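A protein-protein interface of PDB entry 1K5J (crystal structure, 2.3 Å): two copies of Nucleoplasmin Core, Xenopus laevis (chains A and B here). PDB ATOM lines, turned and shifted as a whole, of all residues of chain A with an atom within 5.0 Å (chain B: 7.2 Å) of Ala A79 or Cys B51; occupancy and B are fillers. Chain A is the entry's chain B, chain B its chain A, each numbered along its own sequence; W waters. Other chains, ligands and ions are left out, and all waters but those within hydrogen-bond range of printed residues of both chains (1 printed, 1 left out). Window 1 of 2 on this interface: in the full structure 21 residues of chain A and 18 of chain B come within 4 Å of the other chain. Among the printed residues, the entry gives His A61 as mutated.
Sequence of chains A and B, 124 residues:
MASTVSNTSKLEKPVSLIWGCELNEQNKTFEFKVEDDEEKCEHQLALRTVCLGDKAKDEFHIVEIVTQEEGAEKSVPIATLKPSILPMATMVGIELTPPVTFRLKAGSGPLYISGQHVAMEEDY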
ATOM      1  N   VAL A  50       9.156  34.738  -9.957  1.00  0.00           N
ATOM      2  CA  VAL A  50       9.358  33.549 -10.763  1.00  0.00           C
ATOM      3  C   VAL A  50       7.995  32.870 -10.667  1.00  0.00           C
ATOM      4  O   VAL A  50       7.461  32.710  -9.569  1.00  0.00           O
ATOM      5  CB  VAL A  50      10.415  32.592 -10.179  1.00  0.00           C
ATOM      6  CG1 VAL A  50      10.533  31.371 -11.058  1.00  0.00           C
ATOM      7  CG2 VAL A  50      11.755  33.269 -10.101  1.00  0.00           C
ATOM      8  N   HIS A  61      10.106  22.332 -10.618  1.00  0.00           N
ATOM      9  CA  HIS A  61      10.847  23.170 -11.550  1.00  0.00           C
ATOM     10  C   HIS A  61      11.903  23.869 -10.727  1.00  0.00           C
ATOM     11  O   HIS A  61      11.616  24.397  -9.653  1.00  0.00           O
ATOM     12  CB  HIS A  61       9.937  24.232 -12.191  1.00  0.00           C
ATOM     13  CG  HIS A  61       9.004  23.694 -13.232  1.00  0.00           C
ATOM     14  ND1 HIS A  61       7.995  22.802 -12.937  1.00  0.00           N
ATOM     15  CD2 HIS A  61       8.920  23.929 -14.561  1.00  0.00           C
ATOM     16  CE1 HIS A  61       7.330  22.512 -14.042  1.00  0.00           C
ATOM     17  NE2 HIS A  61       7.872  23.184 -15.042  1.00  0.00           N
ATOM     18  N   ILE A  62      13.133  23.856 -11.212  1.00  0.00           N
ATOM     19  CA  ILE A  62      14.204  24.527 -10.504  1.00  0.00           C
ATOM     20  C   ILE A  62      14.962  25.445 -11.439  1.00  0.00           C
ATOM     21  O   ILE A  62      15.414  25.039 -12.502  1.00  0.00           O
ATOM     22  CB  ILE A  62      15.187  23.524  -9.873  1.00  0.00           C
ATOM     23  CG1 ILE A  62      14.473  22.708  -8.791  1.00  0.00           C
ATOM     24  CG2 ILE A  62      16.366  24.276  -9.289  1.00  0.00           C
ATOM     25  CD1 ILE A  62      15.260  21.523  -8.291  1.00  0.00           C
ATOM     26  N   VAL A  63      15.072  26.703 -11.046  1.00  0.00           N
ATOM     27  CA  VAL A  63      15.810  27.666 -11.830  1.00  0.00           C
ATOM     28  C   VAL A  63      17.042  28.020 -11.019  1.00  0.00           C
ATOM     29  O   VAL A  63      16.967  28.215  -9.806  1.00  0.00           O
ATOM     30  CB  VAL A  63      14.978  28.941 -12.136  1.00  0.00           C
ATOM     31  CG1 VAL A  63      14.352  29.479 -10.878  1.00  0.00           C
ATOM     32  CG2 VAL A  63      15.861  29.998 -12.764  1.00  0.00           C
ATOM     33  N   PRO A  77      21.119  27.424  -7.438  1.00  0.00           N
ATOM     34  CA  PRO A  77      19.657  27.307  -7.439  1.00  0.00           C
ATOM     35  C   PRO A  77      19.040  28.448  -6.625  1.00  0.00           C
ATOM     36  O   PRO A  77      19.485  28.735  -5.513  1.00  0.00           O
ATOM     37  CB  PRO A  77      19.426  25.957  -6.777  1.00  0.00           C
ATOM     38  CG  PRO A  77      20.613  25.175  -7.218  1.00  0.00           C
ATOM     39  CD  PRO A  77      21.743  26.155  -7.036  1.00  0.00           C
ATOM     40  N   ILE A  78      18.027  29.107  -7.178  1.00  0.00           N
ATOM     41  CA  ILE A  78      17.385  30.209  -6.480  1.00  0.00           C
ATOM     42  C   ILE A  78      15.898  29.990  -6.280  1.00  0.00           C
ATOM     43  O   ILE A  78      15.256  30.726  -5.539  1.00  0.00           O
ATOM     44  CB  ILE A  78      17.594  31.541  -7.226  1.00  0.00           C
ATOM     45  CG1 ILE A  78      17.005  31.459  -8.635  1.00  0.00           C
ATOM     46  CG2 ILE A  78      19.071  31.854  -7.303  1.00  0.00           C
ATOM     47  CD1 ILE A  78      16.982  32.784  -9.362  1.00  0.00           C
ATOM     48  N   ALA A  79      15.343  28.975  -6.933  1.00  0.00           N
ATOM     49  CA  ALA A  79      13.918  28.709  -6.788  1.00  0.00           C
ATOM     50  C   ALA A  79      13.477  27.307  -7.186  1.00  0.00           C
ATOM     51  O   ALA A  79      13.951  26.737  -8.168  1.00  0.00           O
ATOM     52  CB  ALA A  79      13.111  29.739  -7.582  1.00  0.00           C
ATOM     53  N   THR A  80      12.554  26.769  -6.396  1.00  0.00           N
ATOM     54  CA  THR A  80      11.968  25.463  -6.651  1.00  0.00           C
ATOM     55  C   THR A  80      10.463  25.656  -6.625  1.00  0.00           C
ATOM     56  O   THR A  80       9.896  26.030  -5.605  1.00  0.00           O
ATOM     57  CB  THR A  80      12.355  24.429  -5.583  1.00  0.00           C
ATOM     58  OG1 THR A  80      13.763  24.215  -5.633  1.00  0.00           O
ATOM     59  CG2 THR A  80      11.628  23.108  -5.829  1.00  0.00           C
ATOM     60  N   LEU A  81       9.828  25.416  -7.762  1.00  0.00           N
ATOM     61  CA  LEU A  81       8.388  25.574  -7.880  1.00  0.00           C
ATOM     62  C   LEU A  81       7.724  24.284  -8.384  1.00  0.00           C
ATOM     63  O   LEU A  81       8.383  23.392  -8.918  1.00  0.00           O
ATOM     64  CB  LEU A  81       8.078  26.721  -8.852  1.00  0.00           C
ATOM     65  CG  LEU A  81       8.671  28.105  -8.543  1.00  0.00           C
ATOM     66  CD1 LEU A  81       8.443  29.055  -9.709  1.00  0.00           C
ATOM     67  CD2 LEU A  81       8.050  28.659  -7.268  1.00  0.00           C
ATOM     68  N   MET A  91      10.966  37.191  -5.511  1.00  0.00           N
ATOM     69  CA  MET A  91      12.406  37.355  -5.315  1.00  0.00           C
ATOM     70  C   MET A  91      12.645  38.712  -4.646  1.00  0.00           C
ATOM     71  O   MET A  91      12.062  39.726  -5.049  1.00  0.00           O
ATOM     72  CB  MET A  91      13.139  37.318  -6.656  1.00  0.00           C
ATOM     73  CG  MET A  91      12.962  36.036  -7.468  1.00  0.00           C
ATOM     74  SD  MET A  91      13.552  34.529  -6.646  1.00  0.00           S
ATOM     75  CE  MET A  91      11.999  33.879  -6.077  1.00  0.00           C
ATOM     76  N   CYS B  21      25.315  27.354  -1.697  1.00  0.00           N
ATOM     77  CA  CYS B  21      25.855  26.099  -1.202  1.00  0.00           C
ATOM     78  C   CYS B  21      24.782  25.035  -1.125  1.00  0.00           C
ATOM     79  O   CYS B  21      23.590  25.334  -1.073  1.00  0.00           O
ATOM     80  CB  CYS B  21      26.489  26.271   0.187  1.00  0.00           C
ATOM     81  SG  CYS B  21      25.347  26.467   1.552  1.00  0.00           S
ATOM     82  N   THR B  49      17.586  32.987  -0.991  1.00  0.00           N
ATOM     83  CA  THR B  49      16.620  31.903  -1.010  1.00  0.00           C
ATOM     84  C   THR B  49      17.178  30.585  -0.500  1.00  0.00           C
ATOM     85  O   THR B  49      18.391  30.367  -0.456  1.00  0.00           O
ATOM     86  CB  THR B  49      16.079  31.624  -2.441  1.00  0.00           C
ATOM     87  OG1 THR B  49      17.170  31.274  -3.298  1.00  0.00           O
ATOM     88  CG2 THR B  49      15.359  32.829  -3.012  1.00  0.00           C
ATOM     89  N   VAL B  50      16.252  29.720  -0.110  1.00  0.00           N
ATOM     90  CA  VAL B  50      16.553  28.368   0.329  1.00  0.00           C
ATOM     91  C   VAL B  50      15.546  27.544  -0.469  1.00  0.00           C
ATOM     92  O   VAL B  50      14.373  27.878  -0.498  1.00  0.00           O
ATOM     93  CB  VAL B  50      16.280  28.147   1.826  1.00  0.00           C
ATOM     94  CG1 VAL B  50      16.585  26.716   2.186  1.00  0.00           C
ATOM     95  CG2 VAL B  50      17.132  29.063   2.658  1.00  0.00           C
ATOM     96  N   CYS B  51      16.008  26.499  -1.136  1.00  0.00           N
ATOM     97  CA  CYS B  51      15.107  25.658  -1.901  1.00  0.00           C
ATOM     98  C   CYS B  51      15.616  24.237  -1.991  1.00  0.00           C
ATOM     99  O   CYS B  51      16.814  23.993  -1.936  1.00  0.00           O
ATOM    100  CB  CYS B  51      14.866  26.241  -3.300  1.00  0.00           C
ATOM    101  SG  CYS B  51      16.305  26.493  -4.335  1.00  0.00           S
ATOM    102  N   LEU B  52      14.687  23.300  -2.126  1.00  0.00           N
ATOM    103  CA  LEU B  52      15.019  21.885  -2.185  1.00  0.00           C
ATOM    104  C   LEU B  52      15.232  21.347  -3.587  1.00  0.00           C
ATOM    105  O   LEU B  52      14.669  21.851  -4.552  1.00  0.00           O
ATOM    106  CB  LEU B  52      13.917  21.080  -1.503  1.00  0.00           C
ATOM    107  CG  LEU B  52      13.581  21.531  -0.079  1.00  0.00           C
ATOM    108  CD1 LEU B  52      12.430  20.693   0.467  1.00  0.00           C
ATOM    109  CD2 LEU B  52      14.821  21.418   0.810  1.00  0.00           C
ATOM    110  N   GLY B  53      16.059  20.317  -3.687  1.00  0.00           N
ATOM    111  CA  GLY B  53      16.303  19.689  -4.969  1.00  0.00           C
ATOM    112  C   GLY B  53      15.081  18.845  -5.281  1.00  0.00           C
ATOM    113  O   GLY B  53      14.375  18.445  -4.361  1.00  0.00           O
ATOM    114  N   LEU B  81      11.461  23.436   5.351  1.00  0.00           N
ATOM    115  CA  LEU B  81      10.908  23.160   4.039  1.00  0.00           C
ATOM    116  C   LEU B  81      10.510  21.687   3.911  1.00  0.00           C
ATOM    117  O   LEU B  81      10.940  20.844   4.699  1.00  0.00           O
ATOM    118  CB  LEU B  81      11.945  23.504   2.962  1.00  0.00           C
ATOM    119  CG  LEU B  81      12.495  24.939   2.913  1.00  0.00           C
ATOM    120  CD1 LEU B  81      13.644  25.042   1.914  1.00  0.00           C
ATOM    121  CD2 LEU B  81      11.382  25.907   2.535  1.00  0.00           C
ATOM    122  N   LEU B  86       6.157  22.914   1.090  1.00  0.00           N
ATOM    123  CA  LEU B  86       6.776  24.210   0.825  1.00  0.00           C
ATOM    124  C   LEU B  86       8.193  23.933   0.320  1.00  0.00           C
ATOM    125  O   LEU B  86       9.132  23.803   1.099  1.00  0.00           O
ATOM    126  CB  LEU B  86       6.813  25.020   2.118  1.00  0.00           C
ATOM    127  CG  LEU B  86       6.801  26.553   2.144  1.00  0.00           C
ATOM    128  CD1 LEU B  86       8.041  27.029   2.826  1.00  0.00           C
ATOM    129  CD2 LEU B  86       6.665  27.137   0.762  1.00  0.00           C
ATOM    130  N   PRO B  87       8.360  23.844  -1.007  1.00  0.00           N
ATOM    131  CA  PRO B  87       9.658  23.562  -1.623  1.00  0.00           C
ATOM    132  C   PRO B  87      10.747  24.636  -1.540  1.00  0.00           C
ATOM    133  O   PRO B  87      11.903  24.353  -1.814  1.00  0.00           O
ATOM    134  CB  PRO B  87       9.274  23.218  -3.061  1.00  0.00           C
ATOM    135  CG  PRO B  87       8.141  24.128  -3.302  1.00  0.00           C
ATOM    136  CD  PRO B  87       7.327  24.017  -2.040  1.00  0.00           C
ATOM    137  N   MET B  88      10.387  25.859  -1.169  1.00  0.00           N
ATOM    138  CA  MET B  88      11.389  26.925  -1.066  1.00  0.00           C
ATOM    139  C   MET B  88      10.921  28.070  -0.178  1.00  0.00           C
ATOM    140  O   MET B  88       9.764  28.131   0.209  1.00  0.00           O
ATOM    141  CB  MET B  88      11.725  27.495  -2.448  1.00  0.00           C
ATOM    142  CG  MET B  88      10.627  28.400  -3.011  1.00  0.00           C
ATOM    143  SD  MET B  88      11.048  29.233  -4.550  1.00  0.00           S
ATOM    144  CE  MET B  88      12.112  30.517  -3.924  1.00  0.00           C
ATOM    145  N   ALA B  89      11.840  28.976   0.125  1.00  0.00           N
ATOM    146  CA  ALA B  89      11.545  30.145   0.937  1.00  0.00           C
ATOM    147  C   ALA B  89      12.473  31.304   0.561  1.00  0.00           C
ATOM    148  O   ALA B  89      13.649  31.109   0.237  1.00  0.00           O
ATOM    149  CB  ALA B  89      11.685  29.814   2.426  1.00  0.00           C
ATOM    150  N   PRO B 110      19.034  17.206  -1.392  1.00  0.00           N
ATOM    151  CA  PRO B 110      19.779  18.454  -1.279  1.00  0.00           C
ATOM    152  C   PRO B 110      18.939  19.677  -0.971  1.00  0.00           C
ATOM    153  O   PRO B 110      17.788  19.765  -1.364  1.00  0.00           O
ATOM    154  CB  PRO B 110      20.481  18.558  -2.631  1.00  0.00           C
ATOM    155  CG  PRO B 110      19.570  17.873  -3.539  1.00  0.00           C
ATOM    156  CD  PRO B 110      19.134  16.668  -2.757  1.00  0.00           C
ATOM    157  N   LEU B 111      19.533  20.597  -0.221  1.00  0.00           N
ATOM    158  CA  LEU B 111      18.907  21.854   0.121  1.00  0.00           C
ATOM    159  C   LEU B 111      19.911  22.902  -0.337  1.00  0.00           C
ATOM    160  O   LEU B 111      21.093  22.835  -0.001  1.00  0.00           O
ATOM    161  CB  LEU B 111      18.659  21.965   1.630  1.00  0.00           C
ATOM    162  CG  LEU B 111      18.072  23.296   2.112  1.00  0.00           C
ATOM    163  CD1 LEU B 111      17.182  23.077   3.305  1.00  0.00           C
ATOM    164  CD2 LEU B 111      19.206  24.280   2.437  1.00  0.00           C
ATOM    165  N   TYR B 112      19.445  23.854  -1.129  1.00  0.00           N
ATOM    166  CA  TYR B 112      20.319  24.900  -1.622  1.00  0.00           C
ATOM    167  C   TYR B 112      20.075  26.214  -0.899  1.00  0.00           C
ATOM    168  O   TYR B 112      18.958  26.537  -0.519  1.00  0.00           O
ATOM    169  CB  TYR B 112      20.121  25.110  -3.126  1.00  0.00           C
ATOM    170  CG  TYR B 112      20.202  23.847  -3.941  1.00  0.00           C
ATOM    171  CD1 TYR B 112      19.056  23.287  -4.500  1.00  0.00           C
ATOM    172  CD2 TYR B 112      21.422  23.204  -4.151  1.00  0.00           C
ATOM    173  CE1 TYR B 112      19.122  22.122  -5.262  1.00  0.00           C
ATOM    174  CE2 TYR B 112      21.501  22.043  -4.903  1.00  0.00           C
ATOM    175  CZ  TYR B 112      20.342  21.504  -5.457  1.00  0.00           C
ATOM    176  OH  TYR B 112      20.402  20.365  -6.212  1.00  0.00           O
ATOM    177  N   ILE B 113      21.143  26.961  -0.693  1.00  0.00           N
ATOM    178  CA  ILE B 113      21.041  28.256  -0.061  1.00  0.00           C
ATOM    179  C   ILE B 113      21.716  29.200  -1.025  1.00  0.00           C
ATOM    180  O   ILE B 113      22.829  28.947  -1.466  1.00  0.00           O
ATOM    181  CB  ILE B 113      21.778  28.311   1.282  1.00  0.00           C
ATOM    182  CG1 ILE B 113      21.277  27.198   2.202  1.00  0.00           C
ATOM    183  CG2 ILE B 113      21.555  29.669   1.922  1.00  0.00           C
ATOM    184  CD1 ILE B 113      21.950  27.185   3.570  1.00  0.00           C
ATOM    185  N   SER B 114      21.031  30.270  -1.388  1.00  0.00           N
ATOM    186  CA  SER B 114      21.609  31.234  -2.307  1.00  0.00           C
ATOM    187  C   SER B 114      21.805  32.540  -1.558  1.00  0.00           C
ATOM    188  O   SER B 114      21.113  32.814  -0.571  1.00  0.00           O
ATOM    189  CB  SER B 114      20.680  31.468  -3.499  1.00  0.00           C
ATOM    190  OG  SER B 114      19.521  32.170  -3.092  1.00  0.00           O
HETATM  191  O   HOH W   1      22.030  27.540  -4.023  1.00  0.00           O
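The side-chain sulfur of Met B88 is in hydrogen-bond range of the backbone NH of Thr A80. O of Leu B52 lies within hydrogen-bond range of OG1 of Thr A80 (2.8 Å). SG of Cys B51 lies close to OG1 of Thr A80. SG of Cys B51 sits at hydrogen-bond distance from N of Ala A79. O of Ile A78 is in hydrogen-bond range of OG1 of Thr B49.
The side-chain hydroxyl (OG) of Ser B114 sits at hydrogen-bond distance from the side-chain hydroxyl (OG1) of Thr B49 (2.5 Å). O of Pro B87 lies within hydrogen-bond range of N of Leu B52 (3.0 Å). The backbone carbonyl oxygen of Cys B51 lies within hydrogen-bond range of the backbone NH of Tyr B112 (2.8 Å). O of Val A63 sits at hydrogen-bond distance from N of Ile A78 (3.0 Å). N of Val A63 is in hydrogen-bond range of O of Ala A79. The backbone carbonyl oxygen (O) of Pro B110 lies within hydrogen-bond range of the backbone NH (N) of Gly B53 (2.9 Å).
Leu B52 touches Ile A62. Ile A62 touches Gly B53. Cys B51 touches Pro A77 (SG to CB, 3.999 Å). Tyr B112 touches Pro A77 (CD1 to CB, 3.5 Å). O of Pro A77 touches CB of Ser B114, 3.6 Å away. O of Ile A78 touches CE of Met B88 (3.5 Å). Ala A79 touches Met B88 (CA to SD, 3.7 Å). O of Thr A80 touches CG of Pro B87, at 3.5 Å. Met A91 touches Met B88 (CE to CE, 3.99 Å).
Of the printed residues of chain B, Ala A79 touches Cys B51 (3.7 Å) and Met B88 (3.7 Å). Printed residues of chain A within 4 Å of Cys B51: Pro A77 (3.999 Å), Ala A79 (3.7 Å) and Thr A80 (3.3 Å). Printed residues of chain B within 4 Å of Met A91: Met B88. Of the printed residues of chain A, Leu B52 touches Ile A62 and Thr A80. Of the printed residues of chain B, Pro A77 touches Cys B51 (3.999 Å), Tyr B112 (3.5 Å) and Ser B114 (3.6 Å). Of the printed residues of chain B, Ile A78 touches Thr B49 (3.0 Å) and Met B88 (3.5 Å). Of the printed residues of chain A, Met B88 touches Ile A78, Ala A79, Thr A80 and Met A91. Pro B110 touches none of the printed residues of chain A. The nearest residue of chain B that does not touch Ala A79 is Thr B49 (4.7 Å).
Of the 10 printed residues of chain A, 6 touch a printed residue of chain B. Printed residues of chain A that touch a printed residue of chain B: Ile A62, Pro A77, Ile A78, Ala A79, Thr A80 and Met A91. Of the 16 printed residues of chain B, 8 touch a printed residue of chain A. Hydrophobic or aromatic side chains of chain B that line the printed part of chain A: Pro B87, Met B88 and Tyr B112. Among the printed residues, 14 pairs touch across the chains.
Positions printed for both chains: 50 and 81.
Water W1 bridges the backbone carbonyl oxygen (O) of Ile B113 (3.0 Å) and the backbone carbonyl oxygen (O) of Pro A77 (3.2 Å).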
